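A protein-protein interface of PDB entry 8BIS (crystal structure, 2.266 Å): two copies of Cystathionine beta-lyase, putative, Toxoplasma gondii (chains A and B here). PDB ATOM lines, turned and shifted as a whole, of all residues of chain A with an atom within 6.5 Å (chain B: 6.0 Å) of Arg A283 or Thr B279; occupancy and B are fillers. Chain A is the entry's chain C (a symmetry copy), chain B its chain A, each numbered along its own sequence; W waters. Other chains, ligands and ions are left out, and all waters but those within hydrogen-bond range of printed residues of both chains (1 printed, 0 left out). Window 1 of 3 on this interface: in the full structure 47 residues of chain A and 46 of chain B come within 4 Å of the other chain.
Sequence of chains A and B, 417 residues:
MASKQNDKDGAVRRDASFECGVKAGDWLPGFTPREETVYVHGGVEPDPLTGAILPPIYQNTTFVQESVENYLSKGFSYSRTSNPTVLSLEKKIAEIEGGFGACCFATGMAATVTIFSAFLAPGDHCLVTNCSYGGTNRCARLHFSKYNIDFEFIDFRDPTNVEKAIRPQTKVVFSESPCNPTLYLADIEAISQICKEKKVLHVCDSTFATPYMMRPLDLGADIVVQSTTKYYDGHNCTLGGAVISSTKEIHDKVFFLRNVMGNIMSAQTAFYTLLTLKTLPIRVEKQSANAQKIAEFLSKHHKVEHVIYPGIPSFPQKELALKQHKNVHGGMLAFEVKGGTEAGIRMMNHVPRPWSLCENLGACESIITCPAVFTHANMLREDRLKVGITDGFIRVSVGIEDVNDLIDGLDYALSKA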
ATOM      1  N   LYS A 230       5.808  10.349   2.465  1.00  0.00           N
ATOM      2  CA  LYS A 230       4.630  10.444   1.617  1.00  0.00           C
ATOM      3  C   LYS A 230       4.650   9.463   0.451  1.00  0.00           C
ATOM      4  O   LYS A 230       3.988   8.423   0.500  1.00  0.00           O
ATOM      5  CB  LYS A 230       4.494  11.870   1.091  1.00  0.00           C
ATOM      6  CG  LYS A 230       3.534  12.705   1.888  1.00  0.00           C
ATOM      7  CD  LYS A 230       4.026  12.923   3.300  1.00  0.00           C
ATOM      8  CE  LYS A 230       2.986  13.649   4.130  1.00  0.00           C
ATOM      9  NZ  LYS A 230       3.589  14.288   5.321  1.00  0.00           N
ATOM     10  N   TYR A 231       5.392   9.793  -0.601  1.00  0.00           N
ATOM     11  CA  TYR A 231       5.392   9.024  -1.838  1.00  0.00           C
ATOM     12  C   TYR A 231       6.633   8.163  -2.008  1.00  0.00           C
ATOM     13  O   TYR A 231       6.545   7.071  -2.578  1.00  0.00           O
ATOM     14  CB  TYR A 231       5.266   9.962  -3.036  1.00  0.00           C
ATOM     15  CG  TYR A 231       3.859  10.433  -3.304  1.00  0.00           C
ATOM     16  CD1 TYR A 231       3.431  11.688  -2.887  1.00  0.00           C
ATOM     17  CD2 TYR A 231       2.957   9.625  -3.984  1.00  0.00           C
ATOM     18  CE1 TYR A 231       2.138  12.123  -3.136  1.00  0.00           C
ATOM     19  CE2 TYR A 231       1.666  10.050  -4.241  1.00  0.00           C
ATOM     20  CZ  TYR A 231       1.261  11.299  -3.814  1.00  0.00           C
ATOM     21  OH  TYR A 231      -0.027  11.721  -4.065  1.00  0.00           O
ATOM     22  N   TYR A 232       7.796   8.647  -1.563  1.00  0.00           N
ATOM     23  CA  TYR A 232       8.981   7.798  -1.519  1.00  0.00           C
ATOM     24  C   TYR A 232       8.670   6.493  -0.802  1.00  0.00           C
ATOM     25  O   TYR A 232       8.956   5.402  -1.307  1.00  0.00           O
ATOM     26  CB  TYR A 232      10.122   8.520  -0.808  1.00  0.00           C
ATOM     27  CG  TYR A 232      10.927   9.472  -1.658  1.00  0.00           C
ATOM     28  CD1 TYR A 232      10.326  10.537  -2.317  1.00  0.00           C
ATOM     29  CD2 TYR A 232      12.298   9.321  -1.777  1.00  0.00           C
ATOM     30  CE1 TYR A 232      11.074  11.414  -3.087  1.00  0.00           C
ATOM     31  CE2 TYR A 232      13.052  10.190  -2.536  1.00  0.00           C
ATOM     32  CZ  TYR A 232      12.439  11.232  -3.189  1.00  0.00           C
ATOM     33  OH  TYR A 232      13.208  12.086  -3.948  1.00  0.00           O
ATOM     34  N   ASP A 233       8.087   6.598   0.393  1.00  0.00           N
ATOM     35  CA  ASP A 233       7.522   5.457   1.098  1.00  0.00           C
ATOM     36  C   ASP A 233       6.287   4.970   0.354  1.00  0.00           C
ATOM     37  O   ASP A 233       6.272   3.859  -0.187  1.00  0.00           O
ATOM     38  CB  ASP A 233       7.171   5.840   2.538  1.00  0.00           C
ATOM     39  CG  ASP A 233       6.764   4.648   3.384  1.00  0.00           C
ATOM     40  OD1 ASP A 233       5.779   3.962   3.043  1.00  0.00           O
ATOM     41  OD2 ASP A 233       7.429   4.406   4.408  1.00  0.00           O
ATOM     42  N   GLY A 234       5.240   5.793   0.328  1.00  0.00           N
ATOM     43  CA  GLY A 234       4.024   5.427  -0.369  1.00  0.00           C
ATOM     44  C   GLY A 234       3.312   4.211   0.170  1.00  0.00           C
ATOM     45  O   GLY A 234       2.350   3.751  -0.450  1.00  0.00           O
ATOM     46  N   HIS A 235       3.746   3.671   1.305  1.00  0.00           N
ATOM     47  CA  HIS A 235       3.121   2.479   1.860  1.00  0.00           C
ATOM     48  C   HIS A 235       2.660   2.690   3.297  1.00  0.00           C
ATOM     49  O   HIS A 235       2.391   1.708   3.996  1.00  0.00           O
ATOM     50  CB  HIS A 235       4.073   1.283   1.794  1.00  0.00           C
ATOM     51  CG  HIS A 235       4.288   0.754   0.411  1.00  0.00           C
ATOM     52  ND1 HIS A 235       5.204   1.304  -0.462  1.00  0.00           N
ATOM     53  CD2 HIS A 235       3.725  -0.288  -0.245  1.00  0.00           C
ATOM     54  CE1 HIS A 235       5.188   0.631  -1.597  1.00  0.00           C
ATOM     55  NE2 HIS A 235       4.302  -0.343  -1.491  1.00  0.00           N
ATOM     56  N   THR A 276      10.760   0.659  -1.306  1.00  0.00           N
ATOM     57  CA  THR A 276       9.536   1.253  -1.837  1.00  0.00           C
ATOM     58  C   THR A 276       9.795   2.236  -2.970  1.00  0.00           C
ATOM     59  O   THR A 276       8.885   2.488  -3.765  1.00  0.00           O
ATOM     60  CB  THR A 276       8.748   1.959  -0.731  1.00  0.00           C
ATOM     61  OG1 THR A 276       9.531   3.030  -0.191  1.00  0.00           O
ATOM     62  CG2 THR A 276       8.391   0.984   0.371  1.00  0.00           C
ATOM     63  N   LEU A 277      11.002   2.795  -3.068  1.00  0.00           N
ATOM     64  CA  LEU A 277      11.293   3.724  -4.153  1.00  0.00           C
ATOM     65  C   LEU A 277      11.261   3.036  -5.507  1.00  0.00           C
ATOM     66  O   LEU A 277      10.980   3.684  -6.523  1.00  0.00           O
ATOM     67  CB  LEU A 277      12.657   4.379  -3.938  1.00  0.00           C
ATOM     68  CG  LEU A 277      12.647   5.795  -3.366  1.00  0.00           C
ATOM     69  CD1 LEU A 277      14.057   6.365  -3.327  1.00  0.00           C
ATOM     70  CD2 LEU A 277      11.718   6.691  -4.176  1.00  0.00           C
ATOM     71  N   LYS A 278      11.539   1.728  -5.539  1.00  0.00           N
ATOM     72  CA  LYS A 278      11.641   1.009  -6.804  1.00  0.00           C
ATOM     73  C   LYS A 278      10.338   1.055  -7.587  1.00  0.00           C
ATOM     74  O   LYS A 278      10.359   1.079  -8.823  1.00  0.00           O
ATOM     75  CB  LYS A 278      12.068  -0.437  -6.541  1.00  0.00           C
ATOM     76  CG  LYS A 278      13.398  -0.545  -5.796  1.00  0.00           C
ATOM     77  CD  LYS A 278      13.936  -1.967  -5.753  1.00  0.00           C
ATOM     78  CE  LYS A 278      13.013  -2.901  -4.985  1.00  0.00           C
ATOM     79  NZ  LYS A 278      13.667  -4.217  -4.705  1.00  0.00           N
ATOM     80  N   THR A 279       9.202   1.088  -6.898  1.00  0.00           N
ATOM     81  CA  THR A 279       7.900   1.104  -7.547  1.00  0.00           C
ATOM     82  C   THR A 279       7.264   2.485  -7.579  1.00  0.00           C
ATOM     83  O   THR A 279       6.075   2.592  -7.893  1.00  0.00           O
ATOM     84  CB  THR A 279       6.954   0.127  -6.853  1.00  0.00           C
ATOM     85  OG1 THR A 279       6.901   0.437  -5.456  1.00  0.00           O
ATOM     86  CG2 THR A 279       7.424  -1.314  -7.052  1.00  0.00           C
ATOM     87  N   LEU A 280       8.014   3.543  -7.260  1.00  0.00           N
ATOM     88  CA  LEU A 280       7.417   4.877  -7.268  1.00  0.00           C
ATOM     89  C   LEU A 280       6.850   5.261  -8.632  1.00  0.00           C
ATOM     90  O   LEU A 280       5.738   5.811  -8.673  1.00  0.00           O
ATOM     91  CB  LEU A 280       8.428   5.919  -6.774  1.00  0.00           C
ATOM     92  CG  LEU A 280       7.808   7.301  -6.524  1.00  0.00           C
ATOM     93  CD1 LEU A 280       8.390   7.934  -5.284  1.00  0.00           C
ATOM     94  CD2 LEU A 280       7.980   8.226  -7.724  1.00  0.00           C
ATOM     95  N   PRO A 281       7.537   5.035  -9.762  1.00  0.00           N
ATOM     96  CA  PRO A 281       6.914   5.379 -11.058  1.00  0.00           C
ATOM     97  C   PRO A 281       5.564   4.717 -11.300  1.00  0.00           C
ATOM     98  O   PRO A 281       4.589   5.416 -11.606  1.00  0.00           O
ATOM     99  CB  PRO A 281       7.970   4.927 -12.072  1.00  0.00           C
ATOM    100  CG  PRO A 281       9.257   5.076 -11.341  1.00  0.00           C
ATOM    101  CD  PRO A 281       8.963   4.696  -9.921  1.00  0.00           C
ATOM    102  N   ILE A 282       5.471   3.389 -11.175  1.00  0.00           N
ATOM    103  CA  ILE A 282       4.199   2.720 -11.445  1.00  0.00           C
ATOM    104  C   ILE A 282       3.152   3.116 -10.410  1.00  0.00           C
ATOM    105  O   ILE A 282       1.971   3.295 -10.738  1.00  0.00           O
ATOM    106  CB  ILE A 282       4.391   1.191 -11.515  1.00  0.00           C
ATOM    107  CG1 ILE A 282       5.098   0.661 -10.266  1.00  0.00           C
ATOM    108  CG2 ILE A 282       5.168   0.808 -12.766  1.00  0.00           C
ATOM    109  CD1 ILE A 282       5.341  -0.832 -10.296  1.00  0.00           C
ATOM    110  N   ARG A 283       3.570   3.282  -9.151  1.00  0.00           N
ATOM    111  CA  ARG A 283       2.644   3.718  -8.110  1.00  0.00           C
ATOM    112  C   ARG A 283       2.052   5.082  -8.442  1.00  0.00           C
ATOM    113  O   ARG A 283       0.837   5.282  -8.359  1.00  0.00           O
ATOM    114  CB  ARG A 283       3.354   3.775  -6.758  1.00  0.00           C
ATOM    115  CG  ARG A 283       3.446   2.452  -6.025  1.00  0.00           C
ATOM    116  CD  ARG A 283       3.823   2.660  -4.563  1.00  0.00           C
ATOM    117  NE  ARG A 283       5.230   3.018  -4.387  1.00  0.00           N
ATOM    118  CZ  ARG A 283       5.654   4.200  -3.951  1.00  0.00           C
ATOM    119  NH1 ARG A 283       4.778   5.148  -3.644  1.00  0.00           N
ATOM    120  NH2 ARG A 283       6.951   4.430  -3.817  1.00  0.00           N
ATOM    121  N   VAL A 284       2.905   6.039  -8.803  1.00  0.00           N
ATOM    122  CA  VAL A 284       2.436   7.394  -9.056  1.00  0.00           C
ATOM    123  C   VAL A 284       1.602   7.436 -10.327  1.00  0.00           C
ATOM    124  O   VAL A 284       0.605   8.160 -10.402  1.00  0.00           O
ATOM    125  CB  VAL A 284       3.627   8.370  -9.110  1.00  0.00           C
ATOM    126  CG1 VAL A 284       3.188   9.728  -9.624  1.00  0.00           C
ATOM    127  CG2 VAL A 284       4.249   8.503  -7.730  1.00  0.00           C
ATOM    128  N   GLU A 285       1.964   6.639 -11.334  1.00  0.00           N
ATOM    129  CA  GLU A 285       1.147   6.574 -12.541  1.00  0.00           C
ATOM    130  C   GLU A 285      -0.254   6.066 -12.223  1.00  0.00           C
ATOM    131  O   GLU A 285      -1.253   6.644 -12.669  1.00  0.00           O
ATOM    132  CB  GLU A 285       1.825   5.692 -13.589  1.00  0.00           C
ATOM    133  CG  GLU A 285       3.004   6.355 -14.290  1.00  0.00           C
ATOM    134  CD  GLU A 285       2.574   7.234 -15.451  1.00  0.00           C
ATOM    135  OE1 GLU A 285       1.352   7.401 -15.652  1.00  0.00           O
ATOM    136  OE2 GLU A 285       3.455   7.754 -16.169  1.00  0.00           O
ATOM    137  N   LYS A 286      -0.347   4.995 -11.429  1.00  0.00           N
ATOM    138  CA  LYS A 286      -1.656   4.439 -11.091  1.00  0.00           C
ATOM    139  C   LYS A 286      -2.462   5.406 -10.224  1.00  0.00           C
ATOM    140  O   LYS A 286      -3.650   5.649 -10.479  1.00  0.00           O
ATOM    141  CB  LYS A 286      -1.480   3.091 -10.391  1.00  0.00           C
ATOM    142  CG  LYS A 286      -2.769   2.484  -9.882  1.00  0.00           C
ATOM    143  CD  LYS A 286      -3.689   2.103 -11.027  1.00  0.00           C
ATOM    144  CE  LYS A 286      -4.989   1.514 -10.498  1.00  0.00           C
ATOM    145  NZ  LYS A 286      -5.904   1.094 -11.596  1.00  0.00           N
ATOM    146  N   GLN A 287      -1.829   5.962  -9.186  1.00  0.00           N
ATOM    147  CA  GLN A 287      -2.495   6.940  -8.335  1.00  0.00           C
ATOM    148  C   GLN A 287      -2.971   8.137  -9.141  1.00  0.00           C
ATOM    149  O   GLN A 287      -4.064   8.655  -8.904  1.00  0.00           O
ATOM    150  CB  GLN A 287      -1.556   7.402  -7.223  1.00  0.00           C
ATOM    151  CG  GLN A 287      -1.261   6.352  -6.177  1.00  0.00           C
ATOM    152  CD  GLN A 287      -0.123   6.754  -5.259  1.00  0.00           C
ATOM    153  OE1 GLN A 287       0.987   7.032  -5.710  1.00  0.00           O
ATOM    154  NE2 GLN A 287      -0.393   6.782  -3.960  1.00  0.00           N
ATOM    155  N   SER A 288      -2.178   8.581 -10.115  1.00  0.00           N
ATOM    156  CA  SER A 288      -2.548   9.769 -10.870  1.00  0.00           C
ATOM    157  C   SER A 288      -3.668   9.481 -11.855  1.00  0.00           C
ATOM    158  O   SER A 288      -4.534  10.332 -12.071  1.00  0.00           O
ATOM    159  CB  SER A 288      -1.333  10.329 -11.595  1.00  0.00           C
ATOM    160  OG  SER A 288      -0.278  10.595 -10.690  1.00  0.00           O
ATOM    161  N   GLY A 362      -0.220  10.159  -0.075  1.00  0.00           N
ATOM    162  CA  GLY A 362       0.741   9.576  -0.988  1.00  0.00           C
ATOM    163  C   GLY A 362       0.904   8.077  -0.900  1.00  0.00           C
ATOM    164  O   GLY A 362       1.850   7.539  -1.488  1.00  0.00           O
ATOM    165  N   ALA A 363       0.014   7.384  -0.206  1.00  0.00           N
ATOM    166  CA  ALA A 363       0.169   5.961   0.036  1.00  0.00           C
ATOM    167  C   ALA A 363      -0.708   5.135  -0.895  1.00  0.00           C
ATOM    168  O   ALA A 363      -1.629   5.639  -1.544  1.00  0.00           O
ATOM    169  CB  ALA A 363      -0.162   5.626   1.491  1.00  0.00           C
ATOM    170  N   CYS A 364      -0.392   3.837  -0.945  1.00  0.00           N
ATOM    171  CA  CYS A 364      -1.198   2.881  -1.695  1.00  0.00           C
ATOM    172  C   CYS A 364      -2.657   2.939  -1.263  1.00  0.00           C
ATOM    173  O   CYS A 364      -3.567   2.784  -2.084  1.00  0.00           O
ATOM    174  CB  CYS A 364      -0.642   1.474  -1.485  1.00  0.00           C
ATOM    175  SG  CYS A 364       0.967   1.180  -2.253  1.00  0.00           S
ATOM    176  N   VAL A 398      -5.109   9.927  -3.350  1.00  0.00           N
ATOM    177  CA  VAL A 398      -5.604   8.793  -4.117  1.00  0.00           C
ATOM    178  C   VAL A 398      -4.575   7.672  -4.073  1.00  0.00           C
ATOM    179  O   VAL A 398      -3.379   7.899  -4.299  1.00  0.00           O
ATOM    180  CB  VAL A 398      -5.919   9.201  -5.565  1.00  0.00           C
ATOM    181  CG1 VAL A 398      -6.511   8.029  -6.324  1.00  0.00           C
ATOM    182  CG2 VAL A 398      -6.877  10.384  -5.577  1.00  0.00           C
ATOM    183  N   GLY A 399      -5.040   6.462  -3.776  1.00  0.00           N
ATOM    184  CA  GLY A 399      -4.211   5.282  -3.771  1.00  0.00           C
ATOM    185  C   GLY A 399      -4.337   4.487  -5.054  1.00  0.00           C
ATOM    186  O   GLY A 399      -4.729   5.004  -6.104  1.00  0.00           O
ATOM    187  N   ILE A 400      -4.002   3.200  -4.962  1.00  0.00           N
ATOM    188  CA  ILE A 400      -3.934   2.331  -6.132  1.00  0.00           C
ATOM    189  C   ILE A 400      -5.020   1.263  -6.115  1.00  0.00           C
ATOM    190  O   ILE A 400      -4.963   0.318  -6.904  1.00  0.00           O
ATOM    191  CB  ILE A 400      -2.543   1.688  -6.276  1.00  0.00           C
ATOM    192  CG1 ILE A 400      -2.239   0.791  -5.080  1.00  0.00           C
ATOM    193  CG2 ILE A 400      -1.467   2.751  -6.416  1.00  0.00           C
ATOM    194  CD1 ILE A 400      -0.903   0.095  -5.180  1.00  0.00           C
ATOM    195  N   TYR B  39      -6.046  -6.395  -3.371  1.00  0.00           N
ATOM    196  CA  TYR B  39      -4.598  -6.428  -3.192  1.00  0.00           C
ATOM    197  C   TYR B  39      -4.139  -5.373  -2.194  1.00  0.00           C
ATOM    198  O   TYR B  39      -3.195  -5.600  -1.430  1.00  0.00           O
ATOM    199  CB  TYR B  39      -3.892  -6.245  -4.532  1.00  0.00           C
ATOM    200  CG  TYR B  39      -3.833  -7.514  -5.341  1.00  0.00           C
ATOM    201  CD1 TYR B  39      -2.770  -8.398  -5.206  1.00  0.00           C
ATOM    202  CD2 TYR B  39      -4.850  -7.842  -6.222  1.00  0.00           C
ATOM    203  CE1 TYR B  39      -2.717  -9.565  -5.941  1.00  0.00           C
ATOM    204  CE2 TYR B  39      -4.805  -9.003  -6.962  1.00  0.00           C
ATOM    205  CZ  TYR B  39      -3.739  -9.861  -6.819  1.00  0.00           C
ATOM    206  OH  TYR B  39      -3.696 -11.027  -7.553  1.00  0.00           O
ATOM    207  N   HIS B 235      10.450  -8.060  -4.534  1.00  0.00           N
ATOM    208  CA  HIS B 235      11.504  -7.103  -4.214  1.00  0.00           C
ATOM    209  C   HIS B 235      12.801  -7.776  -3.780  1.00  0.00           C
ATOM    210  O   HIS B 235      13.694  -7.089  -3.270  1.00  0.00           O
ATOM    211  CB  HIS B 235      11.051  -6.136  -3.116  1.00  0.00           C
ATOM    212  CG  HIS B 235       9.940  -5.219  -3.528  1.00  0.00           C
ATOM    213  ND1 HIS B 235       8.635  -5.642  -3.659  1.00  0.00           N
ATOM    214  CD2 HIS B 235       9.938  -3.898  -3.822  1.00  0.00           C
ATOM    215  CE1 HIS B 235       7.877  -4.623  -4.020  1.00  0.00           C
ATOM    216  NE2 HIS B 235       8.643  -3.552  -4.127  1.00  0.00           N
ATOM    217  N   LEU B 275       3.133  -5.578   2.838  1.00  0.00           N
ATOM    218  CA  LEU B 275       3.508  -4.340   2.165  1.00  0.00           C
ATOM    219  C   LEU B 275       3.633  -4.549   0.658  1.00  0.00           C
ATOM    220  O   LEU B 275       3.066  -3.790  -0.137  1.00  0.00           O
ATOM    221  CB  LEU B 275       4.820  -3.814   2.743  1.00  0.00           C
ATOM    222  CG  LEU B 275       4.846  -2.354   3.183  1.00  0.00           C
ATOM    223  CD1 LEU B 275       3.631  -2.035   4.037  1.00  0.00           C
ATOM    224  CD2 LEU B 275       6.126  -2.069   3.947  1.00  0.00           C
ATOM    225  N   THR B 276       4.368  -5.584   0.248  1.00  0.00           N
ATOM    226  CA  THR B 276       4.707  -5.746  -1.163  1.00  0.00           C
ATOM    227  C   THR B 276       3.530  -6.217  -2.006  1.00  0.00           C
ATOM    228  O   THR B 276       3.486  -5.926  -3.205  1.00  0.00           O
ATOM    229  CB  THR B 276       5.863  -6.732  -1.327  1.00  0.00           C
ATOM    230  OG1 THR B 276       5.478  -8.010  -0.815  1.00  0.00           O
ATOM    231  CG2 THR B 276       7.108  -6.241  -0.597  1.00  0.00           C
ATOM    232  N   LEU B 277       2.584  -6.950  -1.414  1.00  0.00           N
ATOM    233  CA  LEU B 277       1.441  -7.451  -2.165  1.00  0.00           C
ATOM    234  C   LEU B 277       0.551  -6.335  -2.689  1.00  0.00           C
ATOM    235  O   LEU B 277      -0.201  -6.558  -3.645  1.00  0.00           O
ATOM    236  CB  LEU B 277       0.609  -8.385  -1.289  1.00  0.00           C
ATOM    237  CG  LEU B 277       0.745  -9.888  -1.528  1.00  0.00           C
ATOM    238  CD1 LEU B 277      -0.214 -10.649  -0.623  1.00  0.00           C
ATOM    239  CD2 LEU B 277       0.490 -10.223  -2.988  1.00  0.00           C
ATOM    240  N   LYS B 278       0.615  -5.145  -2.082  1.00  0.00           N
ATOM    241  CA  LYS B 278      -0.265  -4.054  -2.488  1.00  0.00           C
ATOM    242  C   LYS B 278       0.028  -3.585  -3.907  1.00  0.00           C
ATOM    243  O   LYS B 278      -0.881  -3.127  -4.610  1.00  0.00           O
ATOM    244  CB  LYS B 278      -0.135  -2.889  -1.508  1.00  0.00           C
ATOM    245  CG  LYS B 278      -0.515  -3.241  -0.084  1.00  0.00           C
ATOM    246  CD  LYS B 278      -0.071  -2.163   0.881  1.00  0.00           C
ATOM    247  CE  LYS B 278      -0.465  -2.515   2.304  1.00  0.00           C
ATOM    248  NZ  LYS B 278      -1.914  -2.266   2.532  1.00  0.00           N
ATOM    249  N   THR B 279       1.280  -3.692  -4.347  1.00  0.00           N
ATOM    250  CA  THR B 279       1.675  -3.263  -5.677  1.00  0.00           C
ATOM    251  C   THR B 279       1.809  -4.421  -6.657  1.00  0.00           C
ATOM    252  O   THR B 279       2.286  -4.209  -7.775  1.00  0.00           O
ATOM    253  CB  THR B 279       2.991  -2.487  -5.611  1.00  0.00           C
ATOM    254  OG1 THR B 279       4.022  -3.338  -5.095  1.00  0.00           O
ATOM    255  CG2 THR B 279       2.848  -1.267  -4.711  1.00  0.00           C
ATOM    256  N   LEU B 280       1.412  -5.637  -6.268  1.00  0.00           N
ATOM    257  CA  LEU B 280       1.533  -6.764  -7.192  1.00  0.00           C
ATOM    258  C   LEU B 280       0.827  -6.505  -8.515  1.00  0.00           C
ATOM    259  O   LEU B 280       1.428  -6.784  -9.565  1.00  0.00           O
ATOM    260  CB  LEU B 280       1.033  -8.059  -6.538  1.00  0.00           C
ATOM    261  CG  LEU B 280       1.207  -9.347  -7.362  1.00  0.00           C
ATOM    262  CD1 LEU B 280       1.492 -10.531  -6.466  1.00  0.00           C
ATOM    263  CD2 LEU B 280      -0.001  -9.651  -8.238  1.00  0.00           C
ATOM    264  N   PRO B 281      -0.412  -6.001  -8.556  1.00  0.00           N
ATOM    265  CA  PRO B 281      -1.032  -5.740  -9.870  1.00  0.00           C
ATOM    266  C   PRO B 281      -0.219  -4.823 -10.769  1.00  0.00           C
ATOM    267  O   PRO B 281       0.054  -5.184 -11.921  1.00  0.00           O
ATOM    268  CB  PRO B 281      -2.385  -5.129  -9.494  1.00  0.00           C
ATOM    269  CG  PRO B 281      -2.700  -5.729  -8.179  1.00  0.00           C
ATOM    270  CD  PRO B 281      -1.395  -5.881  -7.463  1.00  0.00           C
ATOM    271  N   ILE B 282       0.180  -3.643 -10.283  1.00  0.00           N
ATOM    272  CA  ILE B 282       0.902  -2.705 -11.141  1.00  0.00           C
ATOM    273  C   ILE B 282       2.298  -3.231 -11.460  1.00  0.00           C
ATOM    274  O   ILE B 282       2.802  -3.058 -12.581  1.00  0.00           O
ATOM    275  CB  ILE B 282       0.946  -1.306 -10.495  1.00  0.00           C
ATOM    276  CG1 ILE B 282       1.629  -1.345  -9.128  1.00  0.00           C
ATOM    277  CG2 ILE B 282      -0.454  -0.743 -10.347  1.00  0.00           C
ATOM    278  CD1 ILE B 282       1.816   0.032  -8.507  1.00  0.00           C
ATOM    279  N   ARG B 283       2.940  -3.893 -10.495  1.00  0.00           N
ATOM    280  CA  ARG B 283       4.248  -4.489 -10.752  1.00  0.00           C
ATOM    281  C   ARG B 283       4.159  -5.519 -11.866  1.00  0.00           C
ATOM    282  O   ARG B 283       4.983  -5.529 -12.786  1.00  0.00           O
ATOM    283  CB  ARG B 283       4.793  -5.132  -9.476  1.00  0.00           C
ATOM    284  CG  ARG B 283       5.453  -4.171  -8.512  1.00  0.00           C
ATOM    285  CD  ARG B 283       6.216  -4.915  -7.420  1.00  0.00           C
ATOM    286  NE  ARG B 283       5.327  -5.488  -6.408  1.00  0.00           N
ATOM    287  CZ  ARG B 283       5.087  -6.789  -6.270  1.00  0.00           C
ATOM    288  NH1 ARG B 283       5.667  -7.659  -7.078  1.00  0.00           N
ATOM    289  NH2 ARG B 283       4.268  -7.222  -5.321  1.00  0.00           N
ATOM    290  N   VAL B 284       3.152  -6.390 -11.801  1.00  0.00           N
ATOM    291  CA  VAL B 284       3.021  -7.469 -12.771  1.00  0.00           C
ATOM    292  C   VAL B 284       2.613  -6.919 -14.129  1.00  0.00           C
ATOM    293  O   VAL B 284       3.059  -7.414 -15.168  1.00  0.00           O
ATOM    294  CB  VAL B 284       2.027  -8.528 -12.253  1.00  0.00           C
ATOM    295  CG1 VAL B 284       1.585  -9.459 -13.376  1.00  0.00           C
ATOM    296  CG2 VAL B 284       2.660  -9.326 -11.125  1.00  0.00           C
HETATM  297  O   HOH W   1       6.450  -1.477  -3.424  1.00  0.00           O
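The backbone carbonyl oxygen (O) of His B235 is in hydrogen-bond range of the side-chain amino group (NZ) of Lys A278, 3.2 Å away.
The backbone carbonyl oxygen (O) of Thr B276 is in hydrogen-bond range of the guanidinium group (NH2) of Arg B283 (2.6 Å).
The side-chain hydroxyl (OG1) of Thr B279 lies within hydrogen-bond range of the guanidinium group (NE) of Arg B283, 2.8 Å away.
The backbone carbonyl oxygen (O) of Tyr A231 lies within hydrogen-bond range of the guanidinium group (NH1) of Arg A283 (2.8 Å).
The backbone NH (N) of His A235 sits at hydrogen-bond distance from the side-chain carboxylate (OD1) of Asp A233 (2.7 Å).
SG of Cys A364 lies close to NE2 of His A235 (3.7 Å).
NE of Arg A283 lies within hydrogen-bond range of OG1 of Thr A279 (3.3 Å).
O of Leu B275 touches CD2 of His A235 (3.6 Å).
Thr B279 touches His A235 (CG2 to NE2, 3.7 Å).
His B235 touches Thr A279.
Thr A279 touches Arg B283.
Ile B282 touches Ile A282 (CD1 to CG1, 3.8 Å).
CD1 of Ile A282 touches CG of Arg B283, 3.8 Å away.
Arg A283 touches Thr B279 (CG to CG2, 3.99 Å).
CB of Lys A286 touches CG2 of Ile B282 (3.97 Å).
Cys A364 touches Thr B279 (SG to CG2, 3.9 Å).
CD1 of Ile A400 touches O of Lys B278, at 3.3 Å.
Of the printed residues of chain B, Arg A283 touches Thr B279 (3.99 Å) and Ile B282 (3.7 Å).
Ser A288 touches none of the printed residues of chain B.
Printed residues of chain A within 4 Å of Leu B275: His A235.
Of the printed residues of chain A, Lys B278 touches Ile A400.
Printed residues of chain A within 4 Å of Thr B279: His A235, Arg A283 and Cys A364.
Of the printed residues of chain A, Arg B283 touches Thr A279 and Ile A282.
The nearest printed residue of chain A that does not touch Thr B279 is Ile A400 (4.02 Å).
Of the 25 printed residues of chain A, 8 touch a printed residue of chain B.
Hydrophobic or aromatic side chains of chain A within 4 Å of the printed part of chain B: His A235, Ile A282 and Ile A400.
Printed residues of chain B that touch a printed residue of chain A: His B235, Leu B275, Lys B278, Thr B279, Ile B282 and Arg B283.
Among the printed residues, 12 pairs touch across the chains.
His A235 touches Thr B279, and with the chains exchanged Thr A279 touches His B235.
Lys A278 touches His B235, but with the chains exchanged His A235 does not touch Lys B278 (4.4 Å).
Thr A279 touches Arg B283, and with the chains exchanged Arg A283 touches Thr B279.
Ile B282 touches its own counterpart, Ile A282.
10 positions are printed for both chains.
Water W1 lies within hydrogen-bond range of OG1 of Thr A279 (2.8 Å), NE2 of His B235 (3.1 Å), NE2 of His A235 (3.1 Å) and OG1 of Thr B279 (3.5 Å).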
